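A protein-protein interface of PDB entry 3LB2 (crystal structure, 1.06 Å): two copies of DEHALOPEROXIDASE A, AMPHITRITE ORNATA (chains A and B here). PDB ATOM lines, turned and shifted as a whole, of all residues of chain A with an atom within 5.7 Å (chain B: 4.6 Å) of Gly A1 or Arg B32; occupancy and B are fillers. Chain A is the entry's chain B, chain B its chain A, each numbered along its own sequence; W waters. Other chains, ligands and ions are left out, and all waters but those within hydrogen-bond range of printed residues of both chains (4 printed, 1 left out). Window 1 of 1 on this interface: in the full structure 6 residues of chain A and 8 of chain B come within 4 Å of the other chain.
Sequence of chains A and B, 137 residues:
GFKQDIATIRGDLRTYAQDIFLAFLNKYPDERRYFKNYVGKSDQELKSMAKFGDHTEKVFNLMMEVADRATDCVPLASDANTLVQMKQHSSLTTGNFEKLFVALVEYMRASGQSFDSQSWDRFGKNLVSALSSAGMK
The backbone carbonyl oxygen of Tyr B38 sits at hydrogen-bond distance from the guanidinium group of Arg B32, at 3.0 Å.
The guanidinium group (NH1) of Arg B32 lies within hydrogen-bond range of the backbone carbonyl oxygen (O) of Lys B41 (3.4 Å).
The side-chain carboxylate of Asp A5 sits at hydrogen-bond distance from the backbone NH of Asp A116, 2.8 Å away.
N of Gly A1 touches OD1 of Asn B26 (3.7 Å).
NH2 of Arg B32 touches N of Gly A1, at 3.6 Å.
C of Lys B41 touches CB of Lys A3, 3.9 Å away.
Asn B26 touches Ser A114 (CB to OG, 3.7 Å).
OD2 of Asp A116 touches CG of Pro B29, at 3.6 Å.
Of the printed residues of chain B, Gly A1 touches Asn B26 and Arg B32.
Of the printed residues of chain B, Lys A3 touches Lys B41 (3.9 Å).
Printed residues of chain A within 4 Å of Pro B29: Asp A116 (3.6 Å).
Of the printed residues of chain B, Ser A114 touches Asn B26 (3.7 Å).
Phe B35 touches none of the printed residues of chain A.
Val B39 touches none of the printed residues of chain A.
The nearest printed residue of chain B that does not touch Gly A1 is Pro B29 (5.3 Å).
The nearest printed residue of chain A that does not touch Arg B32 is Gln A4 (5.7 Å).
The nearest printed residue of chain B that does not touch Asp A116 is Asp B30 (5.4 Å).
Printed residues of chain B that touch a printed residue of chain A: Asn B26, Pro B29, Arg B32 and Lys B41.
Along chain B the printed residues that touch a printed residue of chain A span positions 26 to 41.
No position is printed for both chains.
Water W3 lies within hydrogen-bond range of the backbone carbonyl oxygen of Asn B26 (2.6 Å), the backbone carbonyl oxygen of Ser A114 (3.1 Å) and the backbone NH of Asp A116 (3.4 Å).
Water W4 lies within hydrogen-bond range of OD1 of Asn B26 (2.8 Å), N of Gly A1 (2.9 Å) and NH2 of Arg B32 (3.1 Å).
Water W2 lies within hydrogen-bond range of the backbone carbonyl oxygen (O) of Leu B25 (2.8 Å), the backbone NH (N) of Gly A1 (2.9 Å) and the guanidinium group (NH2) of Arg B32 (3.1 Å).
Water W1 bridges OD2 of Asp A116 (2.8 Å) and OD1 of Asp B30 (3.1 Å).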
ATOM      1  N   GLY A   1       0.607 -32.836 -24.258  1.00  0.00           N
ATOM      2  CA  GLY A   1      -0.485 -33.234 -25.185  1.00  0.00           C
ATOM      3  C   GLY A   1      -0.171 -34.525 -25.910  1.00  0.00           C
ATOM      4  O   GLY A   1       0.743 -35.260 -25.530  1.00  0.00           O
ATOM      5  N   PHE A   2      -0.927 -34.786 -26.970  1.00  0.00           N
ATOM      6  CA  PHE A   2      -0.807 -36.029 -27.729  1.00  0.00           C
ATOM      7  C   PHE A   2       0.592 -36.201 -28.327  1.00  0.00           C
ATOM      8  O   PHE A   2       1.217 -37.263 -28.185  1.00  0.00           O
ATOM      9  CB  PHE A   2      -1.882 -36.042 -28.815  1.00  0.00           C
ATOM     10  CG  PHE A   2      -1.959 -37.309 -29.624  1.00  0.00           C
ATOM     11  CD1 PHE A   2      -2.547 -38.468 -29.105  1.00  0.00           C
ATOM     12  CD2 PHE A   2      -1.514 -37.322 -30.942  1.00  0.00           C
ATOM     13  CE1 PHE A   2      -2.657 -39.616 -29.880  1.00  0.00           C
ATOM     14  CE2 PHE A   2      -1.623 -38.463 -31.725  1.00  0.00           C
ATOM     15  CZ  PHE A   2      -2.197 -39.607 -31.190  1.00  0.00           C
ATOM     16  N   LYS A   3       1.089 -35.155 -28.988  1.00  0.00           N
ATOM     17  CA  LYS A   3       2.403 -35.225 -29.619  1.00  0.00           C
ATOM     18  C   LYS A   3       3.497 -35.512 -28.605  1.00  0.00           C
ATOM     19  O   LYS A   3       4.380 -36.341 -28.855  1.00  0.00           O
ATOM     20  CB  LYS A   3       2.715 -33.946 -30.388  1.00  0.00           C
ATOM     21  CG  LYS A   3       2.139 -33.908 -31.783  1.00  0.00           C
ATOM     22  CD  LYS A   3       2.818 -34.911 -32.696  1.00  0.00           C
ATOM     23  CE  LYS A   3       2.704 -34.489 -34.139  1.00  0.00           C
ATOM     24  NZ  LYS A   3       3.076 -35.605 -35.040  1.00  0.00           N
ATOM     25  N   GLN A   4       3.448 -34.842 -27.455  1.00  0.00           N
ATOM     26  CA  GLN A   4       4.444 -35.096 -26.426  1.00  0.00           C
ATOM     27  C   GLN A   4       4.297 -36.499 -25.835  1.00  0.00           C
ATOM     28  O   GLN A   4       5.301 -37.145 -25.528  1.00  0.00           O
ATOM     29  CB  GLN A   4       4.409 -34.035 -25.332  1.00  0.00           C
ATOM     30  CG  GLN A   4       5.530 -34.190 -24.304  1.00  0.00           C
ATOM     31  CD  GLN A   4       6.938 -34.164 -24.916  1.00  0.00           C
ATOM     32  OE1 GLN A   4       7.190 -33.507 -25.929  1.00  0.00           O
ATOM     33  NE2 GLN A   4       7.865 -34.869 -24.280  1.00  0.00           N
ATOM     34  N   ASP A   5       3.055 -36.971 -25.685  1.00  0.00           N
ATOM     35  CA  ASP A   5       2.826 -38.325 -25.183  1.00  0.00           C
ATOM     36  C   ASP A   5       3.523 -39.381 -26.045  1.00  0.00           C
ATOM     37  O   ASP A   5       4.016 -40.383 -25.520  1.00  0.00           O
ATOM     38  CB  ASP A   5       1.340 -38.651 -25.140  1.00  0.00           C
ATOM     39  CG  ASP A   5       0.582 -37.904 -24.057  1.00  0.00           C
ATOM     40  OD1 ASP A   5      -0.663 -37.972 -24.141  1.00  0.00           O
ATOM     41  OD2 ASP A   5       1.180 -37.296 -23.130  1.00  0.00           O
ATOM     42  N   ILE A   6       3.529 -39.181 -27.363  1.00  0.00           N
ATOM     43  CA  ILE A   6       4.240 -40.089 -28.251  1.00  0.00           C
ATOM     44  C   ILE A   6       5.719 -40.155 -27.849  1.00  0.00           C
ATOM     45  O   ILE A   6       6.309 -41.239 -27.766  1.00  0.00           O
ATOM     46  CB  ILE A   6       4.085 -39.658 -29.719  1.00  0.00           C
ATOM     47  CG1 ILE A   6       2.609 -39.721 -30.147  1.00  0.00           C
ATOM     48  CG2 ILE A   6       4.952 -40.522 -30.613  1.00  0.00           C
ATOM     49  CD1 ILE A   6       2.316 -39.026 -31.465  1.00  0.00           C
ATOM     50  N   SER A 114       1.335 -37.528 -16.826  1.00  0.00           N
ATOM     51  CA  SER A 114       0.307 -36.589 -17.298  1.00  0.00           C
ATOM     52  C   SER A 114      -0.132 -36.772 -18.756  1.00  0.00           C
ATOM     53  O   SER A 114      -0.139 -35.814 -19.546  1.00  0.00           O
ATOM     54  CB  SER A 114       0.791 -35.153 -17.090  1.00  0.00           C
ATOM     55  OG  SER A 114       1.973 -34.915 -17.836  1.00  0.00           O
ATOM     56  N   ASP A 116      -2.375 -37.147 -22.078  1.00  0.00           N
ATOM     57  CA  ASP A 116      -3.596 -36.527 -22.581  1.00  0.00           C
ATOM     58  C   ASP A 116      -4.538 -37.661 -22.998  1.00  0.00           C
ATOM     59  O   ASP A 116      -4.732 -37.959 -24.186  1.00  0.00           O
ATOM     60  CB  ASP A 116      -3.254 -35.586 -23.733  1.00  0.00           C
ATOM     61  CG  ASP A 116      -4.456 -34.896 -24.323  1.00  0.00           C
ATOM     62  OD1 ASP A 116      -4.247 -34.205 -25.335  1.00  0.00           O
ATOM     63  OD2 ASP A 116      -5.591 -35.038 -23.808  1.00  0.00           O
ATOM     64  N   TRP A 120      -5.939 -39.634 -26.690  1.00  0.00           N
ATOM     65  CA  TRP A 120      -5.757 -41.042 -27.056  1.00  0.00           C
ATOM     66  C   TRP A 120      -7.092 -41.724 -27.307  1.00  0.00           C
ATOM     67  O   TRP A 120      -7.191 -42.583 -28.193  1.00  0.00           O
ATOM     68  CB  TRP A 120      -4.901 -41.780 -26.016  1.00  0.00           C
ATOM     69  CG  TRP A 120      -3.491 -41.300 -26.129  1.00  0.00           C
ATOM     70  CD1 TRP A 120      -2.914 -40.272 -25.440  1.00  0.00           C
ATOM     71  CD2 TRP A 120      -2.512 -41.757 -27.066  1.00  0.00           C
ATOM     72  NE1 TRP A 120      -1.627 -40.072 -25.876  1.00  0.00           N
ATOM     73  CE2 TRP A 120      -1.356 -40.967 -26.879  1.00  0.00           C
ATOM     74  CE3 TRP A 120      -2.502 -42.754 -28.052  1.00  0.00           C
ATOM     75  CZ2 TRP A 120      -0.189 -41.154 -27.634  1.00  0.00           C
ATOM     76  CZ3 TRP A 120      -1.341 -42.939 -28.805  1.00  0.00           C
ATOM     77  CH2 TRP A 120      -0.205 -42.135 -28.591  1.00  0.00           C
ATOM     78  N   LEU B  25      -0.500 -26.800 -19.608  1.00  0.00           N
ATOM     79  CA  LEU B  25      -1.083 -27.504 -20.741  1.00  0.00           C
ATOM     80  C   LEU B  25      -1.192 -29.004 -20.505  1.00  0.00           C
ATOM     81  O   LEU B  25      -2.118 -29.640 -21.015  1.00  0.00           O
ATOM     82  CB  LEU B  25      -0.301 -27.241 -22.015  1.00  0.00           C
ATOM     83  CG  LEU B  25      -0.288 -25.799 -22.527  1.00  0.00           C
ATOM     84  CD1 LEU B  25       0.463 -25.768 -23.839  1.00  0.00           C
ATOM     85  CD2 LEU B  25      -1.693 -25.214 -22.692  1.00  0.00           C
ATOM     86  N   ASN B  26      -0.263 -29.586 -19.755  1.00  0.00           N
ATOM     87  CA  ASN B  26      -0.322 -31.019 -19.478  1.00  0.00           C
ATOM     88  C   ASN B  26      -1.453 -31.374 -18.522  1.00  0.00           C
ATOM     89  O   ASN B  26      -2.088 -32.419 -18.669  1.00  0.00           O
ATOM     90  CB  ASN B  26       1.012 -31.534 -18.940  1.00  0.00           C
ATOM     91  CG  ASN B  26       2.141 -31.421 -19.953  1.00  0.00           C
ATOM     92  OD1 ASN B  26       1.914 -31.245 -21.155  1.00  0.00           O
ATOM     93  ND2 ASN B  26       3.372 -31.517 -19.466  1.00  0.00           N
ATOM     94  N   TYR B  28      -4.203 -29.454 -18.089  1.00  0.00           N
ATOM     95  CA  TYR B  28      -5.441 -29.006 -18.713  1.00  0.00           C
ATOM     96  C   TYR B  28      -5.250 -28.961 -20.225  1.00  0.00           C
ATOM     97  O   TYR B  28      -5.176 -27.883 -20.821  1.00  0.00           O
ATOM     98  CB  TYR B  28      -5.819 -27.624 -18.182  1.00  0.00           C
ATOM     99  CG  TYR B  28      -6.033 -27.584 -16.693  1.00  0.00           C
ATOM    100  CD1 TYR B  28      -7.192 -28.104 -16.125  1.00  0.00           C
ATOM    101  CD2 TYR B  28      -5.080 -27.014 -15.849  1.00  0.00           C
ATOM    102  CE1 TYR B  28      -7.396 -28.071 -14.753  1.00  0.00           C
ATOM    103  CE2 TYR B  28      -5.282 -26.967 -14.475  1.00  0.00           C
ATOM    104  CZ  TYR B  28      -6.438 -27.498 -13.933  1.00  0.00           C
ATOM    105  OH  TYR B  28      -6.626 -27.448 -12.569  1.00  0.00           O
ATOM    106  N   PRO B  29      -5.148 -30.141 -20.863  1.00  0.00           N
ATOM    107  CA  PRO B  29      -4.827 -30.168 -22.292  1.00  0.00           C
ATOM    108  C   PRO B  29      -5.790 -29.395 -23.182  1.00  0.00           C
ATOM    109  O   PRO B  29      -5.377 -28.903 -24.230  1.00  0.00           O
ATOM    110  CB  PRO B  29      -4.835 -31.660 -22.637  1.00  0.00           C
ATOM    111  CG  PRO B  29      -5.513 -32.332 -21.487  1.00  0.00           C
ATOM    112  CD  PRO B  29      -5.267 -31.494 -20.295  1.00  0.00           C
ATOM    113  N   ASP B  30      -7.046 -29.264 -22.763  1.00  0.00           N
ATOM    114  CA  ASP B  30      -8.010 -28.519 -23.558  1.00  0.00           C
ATOM    115  C   ASP B  30      -7.636 -27.037 -23.716  1.00  0.00           C
ATOM    116  O   ASP B  30      -8.079 -26.387 -24.655  1.00  0.00           O
ATOM    117  CB  ASP B  30      -9.430 -28.697 -23.007  1.00  0.00           C
ATOM    118  CG  ASP B  30      -9.986 -30.100 -23.253  1.00  0.00           C
ATOM    119  OD1 ASP B  30      -9.204 -31.070 -23.377  1.00  0.00           O
ATOM    120  OD2 ASP B  30     -11.225 -30.233 -23.318  1.00  0.00           O
ATOM    121  N   GLU B  31      -6.792 -26.523 -22.821  1.00  0.00           N
ATOM    122  CA  GLU B  31      -6.361 -25.118 -22.856  1.00  0.00           C
ATOM    123  C   GLU B  31      -5.465 -24.810 -24.054  1.00  0.00           C
ATOM    124  O   GLU B  31      -5.294 -23.646 -24.423  1.00  0.00           O
ATOM    125  CB  GLU B  31      -5.630 -24.732 -21.561  1.00  0.00           C
ATOM    126  CG  GLU B  31      -6.445 -24.879 -20.280  1.00  0.00           C
ATOM    127  CD  GLU B  31      -7.637 -23.950 -20.218  1.00  0.00           C
ATOM    128  OE1 GLU B  31      -7.443 -22.734 -20.007  1.00  0.00           O
ATOM    129  OE2 GLU B  31      -8.776 -24.442 -20.366  1.00  0.00           O
ATOM    130  N   ARG B  32      -4.883 -25.845 -24.659  1.00  0.00           N
ATOM    131  CA  ARG B  32      -4.005 -25.626 -25.806  1.00  0.00           C
ATOM    132  C   ARG B  32      -4.758 -24.996 -26.984  1.00  0.00           C
ATOM    133  O   ARG B  32      -4.136 -24.355 -27.832  1.00  0.00           O
ATOM    134  CB  ARG B  32      -3.300 -26.917 -26.225  1.00  0.00           C
ATOM    135  CG  ARG B  32      -2.154 -26.684 -27.211  1.00  0.00           C
ATOM    136  CD  ARG B  32      -1.458 -27.973 -27.585  1.00  0.00           C
ATOM    137  NE  ARG B  32      -0.780 -28.596 -26.449  1.00  0.00           N
ATOM    138  CZ  ARG B  32       0.524 -28.867 -26.389  1.00  0.00           C
ATOM    139  NH1 ARG B  32       1.336 -28.544 -27.388  1.00  0.00           N
ATOM    140  NH2 ARG B  32       1.015 -29.462 -25.312  1.00  0.00           N
ATOM    141  N   ARG B  33      -6.087 -25.142 -27.010  1.00  0.00           N
ATOM    142  CA  ARG B  33      -6.919 -24.614 -28.093  1.00  0.00           C
ATOM    143  C   ARG B  33      -6.765 -23.102 -28.275  1.00  0.00           C
ATOM    144  O   ARG B  33      -7.014 -22.569 -29.360  1.00  0.00           O
ATOM    145  CB  ARG B  33      -8.395 -24.983 -27.876  1.00  0.00           C
ATOM    146  CG  ARG B  33      -9.114 -24.230 -26.760  1.00  0.00           C
ATOM    147  CD  ARG B  33     -10.474 -24.862 -26.483  1.00  0.00           C
ATOM    148  NE  ARG B  33     -11.277 -24.101 -25.528  1.00  0.00           N
ATOM    149  CZ  ARG B  33     -11.287 -24.306 -24.213  1.00  0.00           C
ATOM    150  NH1 ARG B  33     -10.528 -25.249 -23.666  1.00  0.00           N
ATOM    151  NH2 ARG B  33     -12.059 -23.557 -23.435  1.00  0.00           N
ATOM    152  N   TYR B  34      -6.366 -22.415 -27.202  1.00  0.00           N
ATOM    153  CA  TYR B  34      -6.187 -20.967 -27.258  1.00  0.00           C
ATOM    154  C   TYR B  34      -4.889 -20.551 -27.930  1.00  0.00           C
ATOM    155  O   TYR B  34      -4.681 -19.367 -28.209  1.00  0.00           O
ATOM    156  CB  TYR B  34      -6.291 -20.363 -25.862  1.00  0.00           C
ATOM    157  CG  TYR B  34      -7.699 -20.409 -25.344  1.00  0.00           C
ATOM    158  CD1 TYR B  34      -8.674 -19.554 -25.860  1.00  0.00           C
ATOM    159  CD2 TYR B  34      -8.073 -21.326 -24.367  1.00  0.00           C
ATOM    160  CE1 TYR B  34      -9.979 -19.596 -25.400  1.00  0.00           C
ATOM    161  CE2 TYR B  34      -9.379 -21.379 -23.901  1.00  0.00           C
ATOM    162  CZ  TYR B  34     -10.325 -20.512 -24.424  1.00  0.00           C
ATOM    163  OH  TYR B  34     -11.618 -20.555 -23.967  1.00  0.00           O
ATOM    164  N   PHE B  35      -4.031 -21.525 -28.209  1.00  0.00           N
ATOM    165  CA  PHE B  35      -2.713 -21.271 -28.763  1.00  0.00           C
ATOM    166  C   PHE B  35      -2.596 -22.078 -30.042  1.00  0.00           C
ATOM    167  O   PHE B  35      -1.969 -23.138 -30.068  1.00  0.00           O
ATOM    168  CB  PHE B  35      -1.647 -21.686 -27.749  1.00  0.00           C
ATOM    169  CG  PHE B  35      -1.858 -21.101 -26.379  1.00  0.00           C
ATOM    170  CD1 PHE B  35      -2.542 -21.811 -25.403  1.00  0.00           C
ATOM    171  CD2 PHE B  35      -1.395 -19.828 -26.072  1.00  0.00           C
ATOM    172  CE1 PHE B  35      -2.759 -21.264 -24.137  1.00  0.00           C
ATOM    173  CE2 PHE B  35      -1.606 -19.280 -24.814  1.00  0.00           C
ATOM    174  CZ  PHE B  35      -2.285 -19.996 -23.845  1.00  0.00           C
ATOM    175  N   LYS B  36      -3.191 -21.564 -31.114  1.00  0.00           N
ATOM    176  CA  LYS B  36      -3.342 -22.356 -32.333  1.00  0.00           C
ATOM    177  C   LYS B  36      -2.008 -22.800 -32.933  1.00  0.00           C
ATOM    178  O   LYS B  36      -1.948 -23.840 -33.595  1.00  0.00           O
ATOM    179  CB  LYS B  36      -4.208 -21.637 -33.370  1.00  0.00           C
ATOM    180  CG  LYS B  36      -3.675 -20.304 -33.857  1.00  0.00           C
ATOM    181  CD  LYS B  36      -4.627 -19.710 -34.874  1.00  0.00           C
ATOM    182  CE  LYS B  36      -4.141 -18.370 -35.380  1.00  0.00           C
ATOM    183  NZ  LYS B  36      -5.063 -17.828 -36.415  1.00  0.00           N
ATOM    184  N   TYR B  38       0.567 -23.784 -31.228  1.00  0.00           N
ATOM    185  CA  TYR B  38       1.178 -24.792 -30.347  1.00  0.00           C
ATOM    186  C   TYR B  38       0.541 -26.179 -30.515  1.00  0.00           C
ATOM    187  O   TYR B  38       1.062 -27.176 -30.005  1.00  0.00           O
ATOM    188  CB  TYR B  38       1.098 -24.383 -28.859  1.00  0.00           C
ATOM    189  CG  TYR B  38       1.738 -23.058 -28.441  1.00  0.00           C
ATOM    190  CD1 TYR B  38       2.633 -22.373 -29.268  1.00  0.00           C
ATOM    191  CD2 TYR B  38       1.468 -22.517 -27.180  1.00  0.00           C
ATOM    192  CE1 TYR B  38       3.213 -21.163 -28.859  1.00  0.00           C
ATOM    193  CE2 TYR B  38       2.040 -21.315 -26.765  1.00  0.00           C
ATOM    194  CZ  TYR B  38       2.908 -20.645 -27.610  1.00  0.00           C
ATOM    195  OH  TYR B  38       3.482 -19.459 -27.204  1.00  0.00           O
ATOM    196  N   VAL B  39      -0.596 -26.234 -31.208  1.00  0.00           N
ATOM    197  CA  VAL B  39      -1.330 -27.481 -31.428  1.00  0.00           C
ATOM    198  C   VAL B  39      -0.492 -28.448 -32.271  1.00  0.00           C
ATOM    199  O   VAL B  39       0.082 -28.050 -33.284  1.00  0.00           O
ATOM    200  CB  VAL B  39      -2.699 -27.191 -32.101  1.00  0.00           C
ATOM    201  CG1 VAL B  39      -3.408 -28.475 -32.521  1.00  0.00           C
ATOM    202  CG2 VAL B  39      -3.589 -26.366 -31.174  1.00  0.00           C
ATOM    203  N   LYS B  41       2.365 -29.961 -31.565  1.00  0.00           N
ATOM    204  CA  LYS B  41       3.806 -29.750 -31.462  1.00  0.00           C
ATOM    205  C   LYS B  41       4.335 -30.385 -30.183  1.00  0.00           C
ATOM    206  O   LYS B  41       3.782 -30.155 -29.106  1.00  0.00           O
ATOM    207  CB  LYS B  41       4.136 -28.249 -31.449  1.00  0.00           C
ATOM    208  CG  LYS B  41       3.481 -27.408 -32.544  1.00  0.00           C
ATOM    209  CD  LYS B  41       4.290 -27.414 -33.833  1.00  0.00           C
ATOM    210  CE  LYS B  41       3.577 -26.657 -34.948  1.00  0.00           C
ATOM    211  NZ  LYS B  41       3.618 -25.179 -34.781  1.00  0.00           N
ATOM    212  N   LEU B  46       8.174 -27.024 -29.778  1.00  0.00           N
ATOM    213  CA  LEU B  46       7.762 -25.735 -29.222  1.00  0.00           C
ATOM    214  C   LEU B  46       8.967 -24.886 -28.877  1.00  0.00           C
ATOM    215  O   LEU B  46       9.026 -23.703 -29.203  1.00  0.00           O
ATOM    216  CB  LEU B  46       6.886 -25.924 -27.981  1.00  0.00           C
ATOM    217  CG  LEU B  46       5.482 -26.459 -28.263  1.00  0.00           C
ATOM    218  CD1 LEU B  46       4.742 -26.758 -26.968  1.00  0.00           C
ATOM    219  CD2 LEU B  46       4.716 -25.459 -29.103  1.00  0.00           C
HETATM  220  O   HOH W   1      -7.495 -33.245 -24.810  1.00  0.00           O
HETATM  221  O   HOH W   2      -1.183 -30.666 -23.427  1.00  0.00           O
HETATM  222  O   HOH W   3      -2.754 -34.373 -20.185  1.00  0.00           O
HETATM  223  O   HOH W   4       2.987 -31.276 -23.689  1.00  0.00           O
